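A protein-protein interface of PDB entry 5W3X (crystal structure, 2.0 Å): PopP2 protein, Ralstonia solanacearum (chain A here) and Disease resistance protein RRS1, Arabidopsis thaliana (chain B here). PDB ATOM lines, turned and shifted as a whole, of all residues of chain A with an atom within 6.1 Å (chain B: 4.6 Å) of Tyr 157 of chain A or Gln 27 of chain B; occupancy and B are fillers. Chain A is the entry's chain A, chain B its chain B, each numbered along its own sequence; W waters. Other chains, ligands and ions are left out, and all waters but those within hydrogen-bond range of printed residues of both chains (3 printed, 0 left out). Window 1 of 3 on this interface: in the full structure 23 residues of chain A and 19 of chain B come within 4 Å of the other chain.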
ATOM      1  N   SER A 123      13.860   0.708  14.905  1.00  0.00           N
ATOM      2  CA  SER A 123      14.988   1.406  15.528  1.00  0.00           C
ATOM      3  C   SER A 123      14.616   1.996  16.892  1.00  0.00           C
ATOM      4  O   SER A 123      15.479   2.300  17.715  1.00  0.00           O
ATOM      5  CB  SER A 123      15.489   2.513  14.597  1.00  0.00           C
ATOM      6  OG  SER A 123      14.516   3.536  14.462  1.00  0.00           O
ATOM      7  N   ARG A 126       7.883   2.856  20.966  1.00  0.00           N
ATOM      8  CA  ARG A 126       6.927   3.816  21.500  1.00  0.00           C
ATOM      9  C   ARG A 126       5.826   3.117  22.274  1.00  0.00           C
ATOM     10  O   ARG A 126       5.700   1.894  22.210  1.00  0.00           O
ATOM     11  CB  ARG A 126       6.307   4.639  20.363  1.00  0.00           C
ATOM     12  CG  ARG A 126       7.334   5.323  19.491  1.00  0.00           C
ATOM     13  CD  ARG A 126       6.663   5.923  18.250  1.00  0.00           C
ATOM     14  NE  ARG A 126       7.594   6.808  17.548  1.00  0.00           N
ATOM     15  CZ  ARG A 126       8.315   6.432  16.498  1.00  0.00           C
ATOM     16  NH1 ARG A 126       8.184   5.201  16.016  1.00  0.00           N
ATOM     17  NH2 ARG A 126       9.145   7.286  15.915  1.00  0.00           N
ATOM     18  N   ASP A 143       5.206   8.767  22.069  1.00  0.00           N
ATOM     19  CA  ASP A 143       6.630   8.555  21.802  1.00  0.00           C
ATOM     20  C   ASP A 143       7.435   9.261  22.878  1.00  0.00           C
ATOM     21  O   ASP A 143       7.305  10.491  23.037  1.00  0.00           O
ATOM     22  CB  ASP A 143       6.969   9.100  20.401  1.00  0.00           C
ATOM     23  CG  ASP A 143       8.399   8.833  19.973  1.00  0.00           C
ATOM     24  OD1 ASP A 143       9.265   8.497  20.812  1.00  0.00           O
ATOM     25  OD2 ASP A 143       8.658   8.964  18.757  1.00  0.00           O
ATOM     26  N   LEU A 145      10.400   9.976  22.918  1.00  0.00           N
ATOM     27  CA  LEU A 145      11.519  10.696  22.347  1.00  0.00           C
ATOM     28  C   LEU A 145      11.010  11.858  21.520  1.00  0.00           C
ATOM     29  O   LEU A 145      10.130  11.688  20.673  1.00  0.00           O
ATOM     30  CB  LEU A 145      12.369   9.783  21.478  1.00  0.00           C
ATOM     31  CG  LEU A 145      13.594  10.395  20.807  1.00  0.00           C
ATOM     32  CD1 LEU A 145      14.651  10.781  21.850  1.00  0.00           C
ATOM     33  CD2 LEU A 145      14.174   9.451  19.746  1.00  0.00           C
ATOM     34  N   LYS A 147      13.128  14.336  19.394  1.00  0.00           N
ATOM     35  CA  LYS A 147      14.475  14.702  18.993  1.00  0.00           C
ATOM     36  C   LYS A 147      14.514  15.608  17.755  1.00  0.00           C
ATOM     37  O   LYS A 147      15.532  16.244  17.488  1.00  0.00           O
ATOM     38  CB  LYS A 147      15.285  13.430  18.743  1.00  0.00           C
ATOM     39  CG  LYS A 147      16.787  13.597  18.836  1.00  0.00           C
ATOM     40  CD  LYS A 147      17.456  12.233  18.698  1.00  0.00           C
ATOM     41  CE  LYS A 147      18.976  12.360  18.623  1.00  0.00           C
ATOM     42  NZ  LYS A 147      19.582  12.978  19.833  1.00  0.00           N
ATOM     43  N   GLU A 148      13.415  15.679  17.005  1.00  0.00           N
ATOM     44  CA  GLU A 148      13.382  16.538  15.823  1.00  0.00           C
ATOM     45  C   GLU A 148      13.460  18.028  16.195  1.00  0.00           C
ATOM     46  O   GLU A 148      12.720  18.502  17.060  1.00  0.00           O
ATOM     47  CB  GLU A 148      12.105  16.271  15.005  1.00  0.00           C
ATOM     48  CG  GLU A 148      12.012  14.864  14.419  1.00  0.00           C
ATOM     49  CD  GLU A 148      12.990  14.639  13.272  1.00  0.00           C
ATOM     50  OE1 GLU A 148      13.105  13.488  12.808  1.00  0.00           O
ATOM     51  OE2 GLU A 148      13.660  15.605  12.836  1.00  0.00           O
ATOM     52  N   ALA A 153       8.349  17.898  11.118  1.00  0.00           N
ATOM     53  CA  ALA A 153       8.794  16.529  10.837  1.00  0.00           C
ATOM     54  C   ALA A 153       7.804  15.494  11.344  1.00  0.00           C
ATOM     55  O   ALA A 153       7.622  14.443  10.723  1.00  0.00           O
ATOM     56  CB  ALA A 153      10.161  16.262  11.444  1.00  0.00           C
ATOM     57  N   TYR A 154       7.159  15.788  12.465  1.00  0.00           N
ATOM     58  CA  TYR A 154       6.313  14.787  13.095  1.00  0.00           C
ATOM     59  C   TYR A 154       5.042  14.492  12.276  1.00  0.00           C
ATOM     60  O   TYR A 154       4.409  13.435  12.452  1.00  0.00           O
ATOM     61  CB  TYR A 154       5.991  15.214  14.522  1.00  0.00           C
ATOM     62  CG  TYR A 154       7.230  15.116  15.417  1.00  0.00           C
ATOM     63  CD1 TYR A 154       7.880  13.894  15.599  1.00  0.00           C
ATOM     64  CD2 TYR A 154       7.755  16.231  16.053  1.00  0.00           C
ATOM     65  CE1 TYR A 154       9.017  13.786  16.406  1.00  0.00           C
ATOM     66  CE2 TYR A 154       8.899  16.134  16.866  1.00  0.00           C
ATOM     67  CZ  TYR A 154       9.520  14.903  17.034  1.00  0.00           C
ATOM     68  OH  TYR A 154      10.649  14.780  17.829  1.00  0.00           O
ATOM     69  N   VAL A 155       4.700  15.393  11.359  1.00  0.00           N
ATOM     70  CA  VAL A 155       3.593  15.108  10.438  1.00  0.00           C
ATOM     71  C   VAL A 155       3.907  13.780   9.773  1.00  0.00           C
ATOM     72  O   VAL A 155       3.085  12.854   9.777  1.00  0.00           O
ATOM     73  CB  VAL A 155       3.402  16.237   9.387  1.00  0.00           C
ATOM     74  CG1 VAL A 155       2.449  15.822   8.260  1.00  0.00           C
ATOM     75  CG2 VAL A 155       2.890  17.490  10.063  1.00  0.00           C
ATOM     76  N   ASP A 156       5.144  13.666   9.288  1.00  0.00           N
ATOM     77  CA  ASP A 156       5.581  12.451   8.621  1.00  0.00           C
ATOM     78  C   ASP A 156       5.410  11.250   9.561  1.00  0.00           C
ATOM     79  O   ASP A 156       4.801  10.245   9.189  1.00  0.00           O
ATOM     80  CB  ASP A 156       7.039  12.571   8.164  1.00  0.00           C
ATOM     81  CG  ASP A 156       7.293  13.806   7.304  1.00  0.00           C
ATOM     82  OD1 ASP A 156       6.318  14.368   6.751  1.00  0.00           O
ATOM     83  OD2 ASP A 156       8.483  14.187   7.160  1.00  0.00           O
ATOM     84  N   TYR A 157       5.908  11.387  10.794  1.00  0.00           N
ATOM     85  CA  TYR A 157       5.879  10.274  11.737  1.00  0.00           C
ATOM     86  C   TYR A 157       4.436   9.837  11.923  1.00  0.00           C
ATOM     87  O   TYR A 157       4.122   8.641  11.885  1.00  0.00           O
ATOM     88  CB  TYR A 157       6.474  10.653  13.099  1.00  0.00           C
ATOM     89  CG  TYR A 157       7.980  10.842  13.198  1.00  0.00           C
ATOM     90  CD1 TYR A 157       8.662  11.727  12.374  1.00  0.00           C
ATOM     91  CD2 TYR A 157       8.707  10.193  14.197  1.00  0.00           C
ATOM     92  CE1 TYR A 157      10.046  11.935  12.516  1.00  0.00           C
ATOM     93  CE2 TYR A 157      10.075  10.386  14.345  1.00  0.00           C
ATOM     94  CZ  TYR A 157      10.744  11.255  13.505  1.00  0.00           C
ATOM     95  OH  TYR A 157      12.111  11.437  13.664  1.00  0.00           O
ATOM     96  N   ALA A 158       3.543  10.816  12.063  1.00  0.00           N
ATOM     97  CA  ALA A 158       2.166  10.486  12.383  1.00  0.00           C
ATOM     98  C   ALA A 158       1.614   9.682  11.211  1.00  0.00           C
ATOM     99  O   ALA A 158       1.040   8.598  11.393  1.00  0.00           O
ATOM    100  CB  ALA A 158       1.358  11.725  12.637  1.00  0.00           C
ATOM    101  N   ASP A 159       1.887  10.178  10.007  1.00  0.00           N
ATOM    102  CA  ASP A 159       1.393   9.519   8.803  1.00  0.00           C
ATOM    103  C   ASP A 159       1.934   8.090   8.766  1.00  0.00           C
ATOM    104  O   ASP A 159       1.190   7.134   8.476  1.00  0.00           O
ATOM    105  CB  ASP A 159       1.799  10.294   7.549  1.00  0.00           C
ATOM    106  CG  ASP A 159       0.893  11.509   7.282  1.00  0.00           C
ATOM    107  OD1 ASP A 159      -0.191  11.613   7.898  1.00  0.00           O
ATOM    108  OD2 ASP A 159       1.271  12.354   6.441  1.00  0.00           O
ATOM    109  N   ASN A 160       3.217   7.943   9.110  1.00  0.00           N
ATOM    110  CA  ASN A 160       3.841   6.615   9.075  1.00  0.00           C
ATOM    111  C   ASN A 160       3.074   5.662   9.963  1.00  0.00           C
ATOM    112  O   ASN A 160       2.697   4.567   9.523  1.00  0.00           O
ATOM    113  CB  ASN A 160       5.314   6.671   9.475  1.00  0.00           C
ATOM    114  CG  ASN A 160       6.157   7.431   8.460  1.00  0.00           C
ATOM    115  OD1 ASN A 160       5.814   7.485   7.275  1.00  0.00           O
ATOM    116  ND2 ASN A 160       7.259   8.026   8.921  1.00  0.00           N
ATOM    117  N   VAL A 161       2.757   6.084  11.186  1.00  0.00           N
ATOM    118  CA  VAL A 161       2.191   5.090  12.083  1.00  0.00           C
ATOM    119  C   VAL A 161       0.793   4.803  11.556  1.00  0.00           C
ATOM    120  O   VAL A 161       0.371   3.634  11.496  1.00  0.00           O
ATOM    121  CB  VAL A 161       2.173   5.535  13.580  1.00  0.00           C
ATOM    122  CG1 VAL A 161       3.557   6.038  14.001  1.00  0.00           C
ATOM    123  CG2 VAL A 161       1.166   6.610  13.830  1.00  0.00           C
ATOM    124  N   ASN A 162       0.133   5.844  11.040  1.00  0.00           N
ATOM    125  CA  ASN A 162      -1.235   5.655  10.584  1.00  0.00           C
ATOM    126  C   ASN A 162      -1.226   4.664   9.441  1.00  0.00           C
ATOM    127  O   ASN A 162      -2.076   3.765   9.389  1.00  0.00           O
ATOM    128  CB  ASN A 162      -1.895   6.967  10.162  1.00  0.00           C
ATOM    129  CG  ASN A 162      -3.434   6.898  10.227  1.00  0.00           C
ATOM    130  OD1 ASN A 162      -4.034   5.820  10.120  1.00  0.00           O
ATOM    131  ND2 ASN A 162      -4.065   8.040  10.418  1.00  0.00           N
ATOM    132  N   PHE A 173      -0.734  10.870  17.243  1.00  0.00           N
ATOM    133  CA  PHE A 173       0.691  10.672  17.503  1.00  0.00           C
ATOM    134  C   PHE A 173       1.193  11.795  18.410  1.00  0.00           C
ATOM    135  O   PHE A 173       1.042  12.990  18.079  1.00  0.00           O
ATOM    136  CB  PHE A 173       1.470  10.628  16.183  1.00  0.00           C
ATOM    137  CG  PHE A 173       2.935  10.418  16.362  1.00  0.00           C
ATOM    138  CD1 PHE A 173       3.463   9.139  16.446  1.00  0.00           C
ATOM    139  CD2 PHE A 173       3.791  11.503  16.494  1.00  0.00           C
ATOM    140  CE1 PHE A 173       4.828   8.954  16.644  1.00  0.00           C
ATOM    141  CE2 PHE A 173       5.142  11.318  16.687  1.00  0.00           C
ATOM    142  CZ  PHE A 173       5.662  10.037  16.766  1.00  0.00           C
ATOM    143  N   LYS B  24      10.359  12.250   6.710  1.00  0.00           N
ATOM    144  CA  LYS B  24      11.059  11.687   7.857  1.00  0.00           C
ATOM    145  C   LYS B  24      10.418  10.392   8.376  1.00  0.00           C
ATOM    146  O   LYS B  24       9.191  10.241   8.378  1.00  0.00           O
ATOM    147  CB  LYS B  24      11.109  12.719   8.974  1.00  0.00           C
ATOM    148  CG  LYS B  24      12.331  12.613   9.858  1.00  0.00           C
ATOM    149  CD  LYS B  24      13.604  12.812   9.063  1.00  0.00           C
ATOM    150  CE  LYS B  24      14.834  12.656   9.939  1.00  0.00           C
ATOM    151  NZ  LYS B  24      14.953  13.733  10.967  1.00  0.00           N
ATOM    152  N   TYR B  25      11.255   9.464   8.820  1.00  0.00           N
ATOM    153  CA  TYR B  25      10.776   8.244   9.458  1.00  0.00           C
ATOM    154  C   TYR B  25      11.302   8.161  10.893  1.00  0.00           C
ATOM    155  O   TYR B  25      10.593   7.749  11.815  1.00  0.00           O
ATOM    156  CB  TYR B  25      11.212   7.012   8.668  1.00  0.00           C
ATOM    157  CG  TYR B  25      10.743   5.697   9.269  1.00  0.00           C
ATOM    158  CD1 TYR B  25      11.511   5.023  10.216  1.00  0.00           C
ATOM    159  CD2 TYR B  25       9.515   5.143   8.904  1.00  0.00           C
ATOM    160  CE1 TYR B  25      11.071   3.820  10.768  1.00  0.00           C
ATOM    161  CE2 TYR B  25       9.071   3.954   9.449  1.00  0.00           C
ATOM    162  CZ  TYR B  25       9.852   3.291  10.376  1.00  0.00           C
ATOM    163  OH  TYR B  25       9.399   2.105  10.912  1.00  0.00           O
ATOM    164  N   GLY B  26      12.549   8.576  11.081  1.00  0.00           N
ATOM    165  CA  GLY B  26      13.155   8.452  12.395  1.00  0.00           C
ATOM    166  C   GLY B  26      14.378   9.324  12.553  1.00  0.00           C
ATOM    167  O   GLY B  26      14.889   9.892  11.589  1.00  0.00           O
ATOM    168  N   GLN B  27      14.860   9.415  13.782  1.00  0.00           N
ATOM    169  CA  GLN B  27      16.013  10.238  14.094  1.00  0.00           C
ATOM    170  C   GLN B  27      16.448   9.836  15.482  1.00  0.00           C
ATOM    171  O   GLN B  27      15.766  10.143  16.455  1.00  0.00           O
ATOM    172  CB  GLN B  27      15.655  11.733  14.030  1.00  0.00           C
ATOM    173  CG  GLN B  27      16.741  12.685  14.502  1.00  0.00           C
ATOM    174  CD  GLN B  27      17.643  13.160  13.380  1.00  0.00           C
ATOM    175  OE1 GLN B  27      17.302  13.055  12.200  1.00  0.00           O
ATOM    176  NE2 GLN B  27      18.806  13.694  13.746  1.00  0.00           N
ATOM    177  N   LYS B  28      17.553   9.108  15.582  1.00  0.00           N
ATOM    178  CA  LYS B  28      17.904   8.540  16.876  1.00  0.00           C
ATOM    179  C   LYS B  28      19.413   8.428  17.106  1.00  0.00           C
ATOM    180  O   LYS B  28      20.181   8.219  16.178  1.00  0.00           O
ATOM    181  CB  LYS B  28      17.247   7.159  17.038  1.00  0.00           C
ATOM    182  CG  LYS B  28      17.123   6.739  18.503  1.00  0.00           C
ATOM    183  CD  LYS B  28      16.317   5.478  18.731  1.00  0.00           C
ATOM    184  CE  LYS B  28      16.127   5.249  20.237  1.00  0.00           C
ATOM    185  NZ  LYS B  28      15.290   4.057  20.557  1.00  0.00           N
ATOM    186  N   PRO B  36      23.920  11.076  15.419  1.00  0.00           N
ATOM    187  CA  PRO B  36      22.631  10.395  15.294  1.00  0.00           C
ATOM    188  C   PRO B  36      22.375   9.916  13.876  1.00  0.00           C
ATOM    189  O   PRO B  36      22.941  10.464  12.927  1.00  0.00           O
ATOM    190  CB  PRO B  36      21.627  11.479  15.687  1.00  0.00           C
ATOM    191  CG  PRO B  36      22.287  12.736  15.269  1.00  0.00           C
ATOM    192  CD  PRO B  36      23.756  12.533  15.545  1.00  0.00           C
ATOM    193  N   ARG B  37      21.536   8.896  13.740  1.00  0.00           N
ATOM    194  CA  ARG B  37      21.114   8.424  12.431  1.00  0.00           C
ATOM    195  C   ARG B  37      19.719   8.938  12.080  1.00  0.00           C
ATOM    196  O   ARG B  37      18.804   8.920  12.912  1.00  0.00           O
ATOM    197  CB  ARG B  37      21.140   6.899  12.382  1.00  0.00           C
ATOM    198  CG  ARG B  37      20.676   6.307  11.063  1.00  0.00           C
ATOM    199  CD  ARG B  37      20.929   4.808  11.055  1.00  0.00           C
ATOM    200  NE  ARG B  37      22.300   4.525  11.463  1.00  0.00           N
ATOM    201  CZ  ARG B  37      22.730   3.336  11.868  1.00  0.00           C
ATOM    202  NH1 ARG B  37      23.999   3.182  12.223  1.00  0.00           N
ATOM    203  NH2 ARG B  37      21.891   2.307  11.938  1.00  0.00           N
ATOM    204  N   GLY B  38      19.577   9.416  10.849  1.00  0.00           N
ATOM    205  CA  GLY B  38      18.296   9.865  10.334  1.00  0.00           C
ATOM    206  C   GLY B  38      17.703   8.857   9.359  1.00  0.00           C
ATOM    207  O   GLY B  38      18.415   8.296   8.520  1.00  0.00           O
ATOM    208  N   TYR B  39      16.403   8.613   9.485  1.00  0.00           N
ATOM    209  CA  TYR B  39      15.704   7.642   8.643  1.00  0.00           C
ATOM    210  C   TYR B  39      14.633   8.351   7.831  1.00  0.00           C
ATOM    211  O   TYR B  39      13.803   9.074   8.402  1.00  0.00           O
ATOM    212  CB  TYR B  39      15.044   6.555   9.482  1.00  0.00           C
ATOM    213  CG  TYR B  39      15.989   5.774  10.381  1.00  0.00           C
ATOM    214  CD1 TYR B  39      16.494   6.337  11.538  1.00  0.00           C
ATOM    215  CD2 TYR B  39      16.321   4.455  10.095  1.00  0.00           C
ATOM    216  CE1 TYR B  39      17.342   5.613  12.392  1.00  0.00           C
ATOM    217  CE2 TYR B  39      17.176   3.727  10.933  1.00  0.00           C
ATOM    218  CZ  TYR B  39      17.671   4.305  12.074  1.00  0.00           C
ATOM    219  OH  TYR B  39      18.509   3.562  12.890  1.00  0.00           O
HETATM  220  O   HOH W   1      13.207  11.099  16.195  1.00  0.00           O
HETATM  221  O   HOH W   2      11.192   6.669  14.341  1.00  0.00           O
HETATM  222  O   HOH W   3       7.885   7.333  11.830  1.00  0.00           O
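OD1 of Asp 143 of chain A lies within hydrogen-bond range of N of Leu 145 of chain A, at 2.8 Å.
O of Gly 26 of chain B sits at hydrogen-bond distance from N of Tyr 39 of chain B.
The side-chain carboxylate (OE1) of Glu 148 of chain A is in hydrogen-bond range of the side-chain hydroxyl (OH) of Tyr 157 of chain A, at 2.4 Å.
N of Arg 37 of chain B lies within hydrogen-bond range of O of Lys 28 of chain B.
The backbone NH (N) of Lys 147 of chain A sits at hydrogen-bond distance from the side-chain hydroxyl (OH) of Tyr 154 of chain A (3.0 Å).
The backbone carbonyl oxygen of Asp 156 of chain A lies close to the side-chain amide nitrogen of Asn 160 of chain A, at 3.3 Å.
Water W2 lies within hydrogen-bond range of the guanidinium group (NH2) of Arg 126 of chain A (2.7 Å) and the backbone carbonyl oxygen (O) of Tyr 25 of chain B (2.8 Å).
Water W3 lies within hydrogen-bond range of the backbone carbonyl oxygen of Tyr 25 of chain B (2.7 Å) and the side-chain amide nitrogen of Asn 160 of chain A (3.1 Å).
Water W1 bridges O of Gln 27 of chain B (2.7 Å) and OH of Tyr 157 of chain A (2.8 Å).
Printed residues of chain B within 4 Å of Ser 123 of chain A: Lys 28 (3.3 Å) and Tyr 39 (3.6 Å).
Of the printed residues of chain B, Glu 148 of chain A touches Lys 24 and Gln 27.
Phe 173 of chain A touches none of the printed residues of chain B.
Printed residues of chain A within 4 Å of Tyr 25 of chain B: Tyr 157 and Asn 160.
Of the printed residues of chain A, Gln 27 of chain B touches Leu 145, Lys 147, Glu 148 and Tyr 157.
Printed residues of chain A within 4 Å of Tyr 39 of chain B: Ser 123.
The nearest printed residue of chain B that does not touch Tyr 157 of chain A is Tyr 39 of chain B (6.0 Å).
The nearest printed residue of chain A that does not touch Tyr 25 of chain B is Arg 126 of chain A (4.4 Å).
Hydrophobic or aromatic side chains of chain B that line the printed part of chain A: Tyr 25 and Tyr 39.
Among the printed residues, 13 pairs touch across the chains.
The side-chain hydroxyl (OH) of Tyr 157 of chain A lies within hydrogen-bond range of the backbone NH (N) of Gln 27 of chain B, 3.4 Å away.
ND2 of Asn 160 of chain A sits at hydrogen-bond distance from O of Lys 24 of chain B (3.0 Å).
The side-chain amino group (NZ) of Lys 28 of chain B sits at hydrogen-bond distance from the backbone carbonyl oxygen (O) of Ser 123 of chain A (3.3 Å).
The side-chain carboxylate (OD2) of Asp 156 of chain A sits at hydrogen-bond distance from the backbone NH (N) of Lys 24 of chain B, at 2.7 Å.
The side-chain carboxylate of Glu 148 of chain A lies within salt-bridge range of the side-chain amino group of Lys 24 of chain B (2.6 Å).
Among the printed residues, merely in contact across the chains: Tyr 157 of chain A with Gly 26 of chain B (3.3 Å), Glu 148 of chain A with Gln 27 of chain B (3.3 Å), Lys 147 of chain A with Gln 27 of chain B (3.5 Å), Asn 160 of chain A with Tyr 25 of chain B (3.6 Å), Tyr 157 of chain A with Lys 24 of chain B (3.6 Å), Ser 123 of chain A with Tyr 39 of chain B (3.6 Å), Tyr 157 of chain A with Tyr 25 of chain B (3.7 Å) and Leu 145 of chain A with Gln 27 of chain B (3.7 Å).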
